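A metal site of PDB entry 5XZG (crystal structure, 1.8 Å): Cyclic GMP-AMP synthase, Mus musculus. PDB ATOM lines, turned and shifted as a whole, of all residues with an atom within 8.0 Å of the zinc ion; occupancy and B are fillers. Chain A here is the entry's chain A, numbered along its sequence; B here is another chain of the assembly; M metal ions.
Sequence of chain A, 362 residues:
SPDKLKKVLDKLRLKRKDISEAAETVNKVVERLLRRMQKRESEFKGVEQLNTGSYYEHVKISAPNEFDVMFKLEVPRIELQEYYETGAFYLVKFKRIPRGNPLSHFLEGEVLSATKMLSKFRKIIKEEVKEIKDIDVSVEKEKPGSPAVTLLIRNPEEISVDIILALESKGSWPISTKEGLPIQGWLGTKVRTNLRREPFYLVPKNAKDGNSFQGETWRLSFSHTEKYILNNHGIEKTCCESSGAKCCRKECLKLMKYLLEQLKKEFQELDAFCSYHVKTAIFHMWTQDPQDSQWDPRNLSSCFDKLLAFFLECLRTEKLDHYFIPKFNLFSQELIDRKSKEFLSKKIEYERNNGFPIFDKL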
ATOM      1  N   LEU A 230      -4.046 -10.989  10.428  1.00  0.00           N
ATOM      2  CA  LEU A 230      -2.590 -10.888  10.327  1.00  0.00           C
ATOM      3  C   LEU A 230      -2.100 -10.219   9.017  1.00  0.00           C
ATOM      4  O   LEU A 230      -1.102  -9.486   9.018  1.00  0.00           O
ATOM      5  CB  LEU A 230      -1.969 -12.288  10.443  1.00  0.00           C
ATOM      6  CG  LEU A 230      -1.505 -12.736  11.844  1.00  0.00           C
ATOM      7  CD1 LEU A 230      -0.340 -11.853  12.292  1.00  0.00           C
ATOM      8  CD2 LEU A 230      -2.620 -12.655  12.816  1.00  0.00           C
ATOM      9  N   ASN A 231      -2.801 -10.486   7.911  1.00  0.00           N
ATOM     10  CA  ASN A 231      -2.516  -9.833   6.633  1.00  0.00           C
ATOM     11  C   ASN A 231      -3.081  -8.397   6.529  1.00  0.00           C
ATOM     12  O   ASN A 231      -2.695  -7.656   5.631  1.00  0.00           O
ATOM     13  CB  ASN A 231      -3.054 -10.685   5.482  1.00  0.00           C
ATOM     14  CG  ASN A 231      -2.323 -10.407   4.153  1.00  0.00           C
ATOM     15  OD1 ASN A 231      -1.089 -10.419   4.102  1.00  0.00           O
ATOM     16  ND2 ASN A 231      -3.087 -10.143   3.087  1.00  0.00           N
ATOM     17  N   ASN A 232      -3.977  -8.025   7.444  1.00  0.00           N
ATOM     18  CA  ASN A 232      -4.666  -6.717   7.449  1.00  0.00           C
ATOM     19  C   ASN A 232      -4.719  -6.095   8.836  1.00  0.00           C
ATOM     20  O   ASN A 232      -5.781  -5.897   9.398  1.00  0.00           O
ATOM     21  CB  ASN A 232      -6.103  -6.849   6.922  1.00  0.00           C
ATOM     22  CG  ASN A 232      -6.141  -7.414   5.529  1.00  0.00           C
ATOM     23  OD1 ASN A 232      -6.052  -6.662   4.539  1.00  0.00           O
ATOM     24  ND2 ASN A 232      -6.240  -8.742   5.438  1.00  0.00           N
ATOM     25  N   HIS A 233      -3.547  -5.796   9.382  1.00  0.00           N
ATOM     26  CA  HIS A 233      -3.394  -5.656  10.835  1.00  0.00           C
ATOM     27  C   HIS A 233      -3.217  -4.227  11.291  1.00  0.00           C
ATOM     28  O   HIS A 233      -3.045  -3.994  12.489  1.00  0.00           O
ATOM     29  CB  HIS A 233      -2.174  -6.457  11.300  1.00  0.00           C
ATOM     30  CG  HIS A 233      -0.914  -6.027  10.605  1.00  0.00           C
ATOM     31  ND1 HIS A 233      -0.276  -6.816   9.682  1.00  0.00           N
ATOM     32  CD2 HIS A 233      -0.242  -4.857  10.649  1.00  0.00           C
ATOM     33  CE1 HIS A 233       0.785  -6.163   9.203  1.00  0.00           C
ATOM     34  NE2 HIS A 233       0.814  -4.986   9.767  1.00  0.00           N
ATOM     35  N   GLY A 234      -3.245  -3.276  10.362  1.00  0.00           N
ATOM     36  CA  GLY A 234      -2.993  -1.885  10.691  1.00  0.00           C
ATOM     37  C   GLY A 234      -4.267  -1.071  10.877  1.00  0.00           C
ATOM     38  O   GLY A 234      -5.304  -1.400  10.293  1.00  0.00           O
ATOM     39  N   ILE A 235      -4.206  -0.011  11.676  1.00  0.00           N
ATOM     40  CA  ILE A 235      -5.297   0.943  11.674  1.00  0.00           C
ATOM     41  C   ILE A 235      -5.271   1.711  10.340  1.00  0.00           C
ATOM     42  O   ILE A 235      -6.319   2.036   9.809  1.00  0.00           O
ATOM     43  CB  ILE A 235      -5.266   1.914  12.879  1.00  0.00           C
ATOM     44  CG1 ILE A 235      -6.551   2.732  12.908  1.00  0.00           C
ATOM     45  CG2 ILE A 235      -4.047   2.832  12.833  1.00  0.00           C
ATOM     46  CD1 ILE A 235      -6.798   3.405  14.240  1.00  0.00           C
ATOM     47  N   GLU A 236      -4.085   1.965   9.792  1.00  0.00           N
ATOM     48  CA  GLU A 236      -4.013   2.560   8.454  1.00  0.00           C
ATOM     49  C   GLU A 236      -4.026   1.457   7.401  1.00  0.00           C
ATOM     50  O   GLU A 236      -3.406   0.411   7.600  1.00  0.00           O
ATOM     51  CB  GLU A 236      -2.754   3.427   8.297  1.00  0.00           C
ATOM     52  CG  GLU A 236      -2.778   4.669   9.169  1.00  0.00           C
ATOM     53  CD  GLU A 236      -1.715   5.671   8.757  1.00  0.00           C
ATOM     54  OE1 GLU A 236      -1.091   5.459   7.694  1.00  0.00           O
ATOM     55  OE2 GLU A 236      -1.490   6.661   9.487  1.00  0.00           O
ATOM     56  N   THR A 238      -2.602   1.307   4.592  1.00  0.00           N
ATOM     57  CA  THR A 238      -1.295   1.097   3.952  1.00  0.00           C
ATOM     58  C   THR A 238      -0.213   0.466   4.866  1.00  0.00           C
ATOM     59  O   THR A 238       0.942   0.324   4.453  1.00  0.00           O
ATOM     60  CB  THR A 238      -0.751   2.416   3.405  1.00  0.00           C
ATOM     61  OG1 THR A 238      -0.614   3.334   4.493  1.00  0.00           O
ATOM     62  CG2 THR A 238      -1.737   3.021   2.345  1.00  0.00           C
ATOM     63  N   CYS A 239      -0.568   0.093   6.102  1.00  0.00           N
ATOM     64  CA  CYS A 239       0.389  -0.530   7.014  1.00  0.00           C
ATOM     65  C   CYS A 239       1.084  -1.743   6.374  1.00  0.00           C
ATOM     66  O   CYS A 239       0.431  -2.678   5.894  1.00  0.00           O
ATOM     67  CB  CYS A 239      -0.315  -0.944   8.305  1.00  0.00           C
ATOM     68  SG  CYS A 239       0.799  -1.437   9.663  1.00  0.00           S
ATOM     69  N   CYS A 240       2.409  -1.682   6.348  1.00  0.00           N
ATOM     70  CA  CYS A 240       3.274  -2.704   5.766  1.00  0.00           C
ATOM     71  C   CYS A 240       3.087  -2.923   4.258  1.00  0.00           C
ATOM     72  O   CYS A 240       3.575  -3.916   3.723  1.00  0.00           O
ATOM     73  CB  CYS A 240       3.097  -4.043   6.509  1.00  0.00           C
ATOM     74  SG  CYS A 240       3.789  -4.021   8.179  1.00  0.00           S
ATOM     75  N   GLU A 241       2.441  -1.984   3.564  1.00  0.00           N
ATOM     76  CA  GLU A 241       2.357  -2.068   2.100  1.00  0.00           C
ATOM     77  C   GLU A 241       3.495  -1.316   1.419  1.00  0.00           C
ATOM     78  O   GLU A 241       4.236  -0.585   2.081  1.00  0.00           O
ATOM     79  CB  GLU A 241       1.012  -1.501   1.593  1.00  0.00           C
ATOM     80  CG  GLU A 241      -0.266  -2.337   1.910  1.00  0.00           C
ATOM     81  CD  GLU A 241      -1.535  -1.717   1.290  1.00  0.00           C
ATOM     82  OE1 GLU A 241      -1.461  -0.554   0.868  1.00  0.00           O
ATOM     83  OE2 GLU A 241      -2.592  -2.392   1.184  1.00  0.00           O
ATOM     84  N   ALA A 245       3.959   2.447   5.646  1.00  0.00           N
ATOM     85  CA  ALA A 245       5.052   2.279   6.598  1.00  0.00           C
ATOM     86  C   ALA A 245       5.031   0.892   7.226  1.00  0.00           C
ATOM     87  O   ALA A 245       3.967   0.404   7.614  1.00  0.00           O
ATOM     88  CB  ALA A 245       4.990   3.342   7.687  1.00  0.00           C
ATOM     89  N   LYS A 246       6.207   0.269   7.316  1.00  0.00           N
ATOM     90  CA  LYS A 246       6.410  -0.980   8.061  1.00  0.00           C
ATOM     91  C   LYS A 246       6.138  -0.773   9.539  1.00  0.00           C
ATOM     92  O   LYS A 246       6.590   0.225  10.120  1.00  0.00           O
ATOM     93  CB  LYS A 246       7.848  -1.486   7.894  1.00  0.00           C
ATOM     94  CG  LYS A 246       8.055  -2.564   6.838  1.00  0.00           C
ATOM     95  CD  LYS A 246       7.502  -3.915   7.277  1.00  0.00           C
ATOM     96  CE  LYS A 246       8.257  -4.464   8.458  1.00  0.00           C
ATOM     97  NZ  LYS A 246       7.637  -5.723   8.978  1.00  0.00           N
ATOM     98  N   CYS A 247       5.440  -1.724  10.148  1.00  0.00           N
ATOM     99  CA  CYS A 247       5.281  -1.765  11.617  1.00  0.00           C
ATOM    100  C   CYS A 247       5.998  -2.984  12.168  1.00  0.00           C
ATOM    101  O   CYS A 247       6.446  -3.826  11.398  1.00  0.00           O
ATOM    102  CB  CYS A 247       3.806  -1.810  12.004  1.00  0.00           C
ATOM    103  SG  CYS A 247       3.005  -3.423  11.794  1.00  0.00           S
ATOM    104  N   CYS A 248       6.081  -3.113  13.490  1.00  0.00           N
ATOM    105  CA  CYS A 248       6.756  -4.277  14.108  1.00  0.00           C
ATOM    106  C   CYS A 248       5.790  -5.275  14.778  1.00  0.00           C
ATOM    107  O   CYS A 248       6.229  -6.142  15.544  1.00  0.00           O
ATOM    108  CB  CYS A 248       7.784  -3.796  15.135  1.00  0.00           C
ATOM    109  SG  CYS A 248       7.076  -3.041  16.629  1.00  0.00           S
ATOM    110  N   ARG A 249       4.498  -5.174  14.500  1.00  0.00           N
ATOM    111  CA  ARG A 249       3.535  -6.113  15.102  1.00  0.00           C
ATOM    112  C   ARG A 249       3.907  -7.591  14.899  1.00  0.00           C
ATOM    113  O   ARG A 249       3.900  -8.361  15.849  1.00  0.00           O
ATOM    114  CB  ARG A 249       2.134  -5.882  14.527  1.00  0.00           C
ATOM    115  CG  ARG A 249       1.484  -4.577  14.923  1.00  0.00           C
ATOM    116  CD  ARG A 249       0.019  -4.562  14.479  1.00  0.00           C
ATOM    117  NE  ARG A 249      -0.713  -3.369  14.920  1.00  0.00           N
ATOM    118  CZ  ARG A 249      -0.756  -2.220  14.233  1.00  0.00           C
ATOM    119  NH1 ARG A 249      -0.053  -2.066  13.111  1.00  0.00           N
ATOM    120  NH2 ARG A 249      -1.482  -1.191  14.679  1.00  0.00           N
ATOM    121  N   LYS A 250       4.196  -7.978  13.661  1.00  0.00           N
ATOM    122  CA  LYS A 250       4.486  -9.374  13.384  1.00  0.00           C
ATOM    123  C   LYS A 250       5.835  -9.805  13.977  1.00  0.00           C
ATOM    124  O   LYS A 250       5.981 -10.943  14.397  1.00  0.00           O
ATOM    125  CB  LYS A 250       4.472  -9.656  11.886  1.00  0.00           C
ATOM    126  CG  LYS A 250       3.081  -9.908  11.320  1.00  0.00           C
ATOM    127  CD  LYS A 250       3.187 -10.169   9.809  1.00  0.00           C
ATOM    128  CE  LYS A 250       1.827 -10.421   9.168  1.00  0.00           C
ATOM    129  NZ  LYS A 250       1.906 -10.440   7.684  1.00  0.00           N
ATOM    130  N   GLU A 251       6.794  -8.879  14.007  1.00  0.00           N
ATOM    131  CA  GLU A 251       8.094  -9.184  14.594  1.00  0.00           C
ATOM    132  C   GLU A 251       7.959  -9.450  16.097  1.00  0.00           C
ATOM    133  O   GLU A 251       8.634 -10.312  16.648  1.00  0.00           O
ATOM    134  CB  GLU A 251       9.080  -8.046  14.332  1.00  0.00           C
ATOM    135  CG  GLU A 251       9.588  -7.953  12.890  1.00  0.00           C
ATOM    136  CD  GLU A 251       8.552  -7.395  11.910  1.00  0.00           C
ATOM    137  OE1 GLU A 251       8.822  -7.436  10.686  1.00  0.00           O
ATOM    138  OE2 GLU A 251       7.486  -6.907  12.347  1.00  0.00           O
ATOM    139  N   ASP A 292      -0.809   2.657  14.668  1.00  0.00           N
ATOM    140  CA  ASP A 292       0.348   2.089  13.985  1.00  0.00           C
ATOM    141  C   ASP A 292       1.605   2.708  14.573  1.00  0.00           C
ATOM    142  O   ASP A 292       2.638   2.054  14.695  1.00  0.00           O
ATOM    143  CB  ASP A 292       0.280   2.334  12.461  1.00  0.00           C
ATOM    144  CG  ASP A 292      -0.847   1.536  11.789  1.00  0.00           C
ATOM    145  OD1 ASP A 292      -1.365   0.589  12.407  1.00  0.00           O
ATOM    146  OD2 ASP A 292      -1.233   1.853  10.637  1.00  0.00           O
ATOM    147  N   TRP A 295       3.472   0.891  17.083  1.00  0.00           N
ATOM    148  CA  TRP A 295       4.253  -0.268  16.665  1.00  0.00           C
ATOM    149  C   TRP A 295       5.257   0.112  15.597  1.00  0.00           C
ATOM    150  O   TRP A 295       5.496  -0.640  14.652  1.00  0.00           O
ATOM    151  CB  TRP A 295       3.330  -1.369  16.174  1.00  0.00           C
ATOM    152  CG  TRP A 295       2.321  -1.762  17.184  1.00  0.00           C
ATOM    153  CD1 TRP A 295       1.103  -1.154  17.404  1.00  0.00           C
ATOM    154  CD2 TRP A 295       2.403  -2.837  18.132  1.00  0.00           C
ATOM    155  NE1 TRP A 295       0.442  -1.807  18.424  1.00  0.00           N
ATOM    156  CE2 TRP A 295       1.215  -2.837  18.888  1.00  0.00           C
ATOM    157  CE3 TRP A 295       3.378  -3.817  18.416  1.00  0.00           C
ATOM    158  CZ2 TRP A 295       0.978  -3.764  19.918  1.00  0.00           C
ATOM    159  CZ3 TRP A 295       3.126  -4.734  19.428  1.00  0.00           C
ATOM    160  CH2 TRP A 295       1.939  -4.693  20.164  1.00  0.00           C
ATOM    161  P    DA B  11       4.653  -9.655   5.308  1.00  0.00           P
ATOM    162  OP1  DA B  11       4.404 -10.483   6.433  1.00  0.00           O
ATOM    163  OP2  DA B  11       4.666  -8.233   5.456  1.00  0.00           O
ATOM    164  O5'  DA B  11       6.038 -10.119   4.728  1.00  0.00           O
ATOM    165  C5'  DA B  11       6.210 -11.494   4.421  1.00  0.00           C
ATOM    166  C4'  DA B  11       7.505 -11.719   3.672  1.00  0.00           C
ATOM    167  O4'  DA B  11       7.394 -11.194   2.340  1.00  0.00           O
ATOM    168  C3'  DA B  11       8.734 -11.047   4.275  1.00  0.00           C
ATOM    169  O3'  DA B  11       9.836 -11.916   4.042  1.00  0.00           O
ATOM    170  C2'  DA B  11       8.963  -9.868   3.341  1.00  0.00           C
ATOM    171  C1'  DA B  11       8.594 -10.547   2.051  1.00  0.00           C
ATOM    172  N9   DA B  11       8.374  -9.667   0.916  1.00  0.00           N
ATOM    173  C8   DA B  11       7.902  -8.376   0.902  1.00  0.00           C
ATOM    174  N7   DA B  11       7.860  -7.842  -0.291  1.00  0.00           N
ATOM    175  C5   DA B  11       8.356  -8.833  -1.121  1.00  0.00           C
ATOM    176  C6   DA B  11       8.575  -8.886  -2.499  1.00  0.00           C
ATOM    177  N6   DA B  11       8.304  -7.882  -3.331  1.00  0.00           N
ATOM    178  N1   DA B  11       9.071 -10.024  -3.016  1.00  0.00           N
ATOM    179  C2   DA B  11       9.350 -11.038  -2.178  1.00  0.00           C
ATOM    180  N3   DA B  11       9.194 -11.102  -0.862  1.00  0.00           N
ATOM    181  C4   DA B  11       8.686  -9.954  -0.387  1.00  0.00           C
HETATM  182 ZN    ZN M   1       2.041  -3.340   9.605  1.00  0.00          ZN
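The zinc ion is bound by a ring nitrogen (NE2) of His 233, the side-chain sulfur of Cys 239, the side-chain sulfur of Cys 240 and the side-chain sulfur of Cys 247.
The zinc ion has four donor atoms within binding distance.
The backbone carbonyl oxygen of His 233 lies close to the guanidinium group of Arg 249, at 3.4 Å.
O of Leu 230 lies within hydrogen-bond range of ND1 of His 233.
The guanidinium group (NH1) of Arg 249 sits close to the side-chain sulfur (SG) of Cys 239, 3.6 Å away.
The backbone NH (N) of Cys 240 lies within hydrogen-bond range of the backbone carbonyl oxygen (O) of Ala 245, 2.9 Å away.
The backbone NH (N) of Arg 249 lies close to the side-chain sulfur (SG) of Cys 247 (3.6 Å).
Of the 21 residues printed, 4 come within 4 Å of the zinc ion.
The nearest printed residue that does not touch the zinc ion is Arg 249 (4.3 Å).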
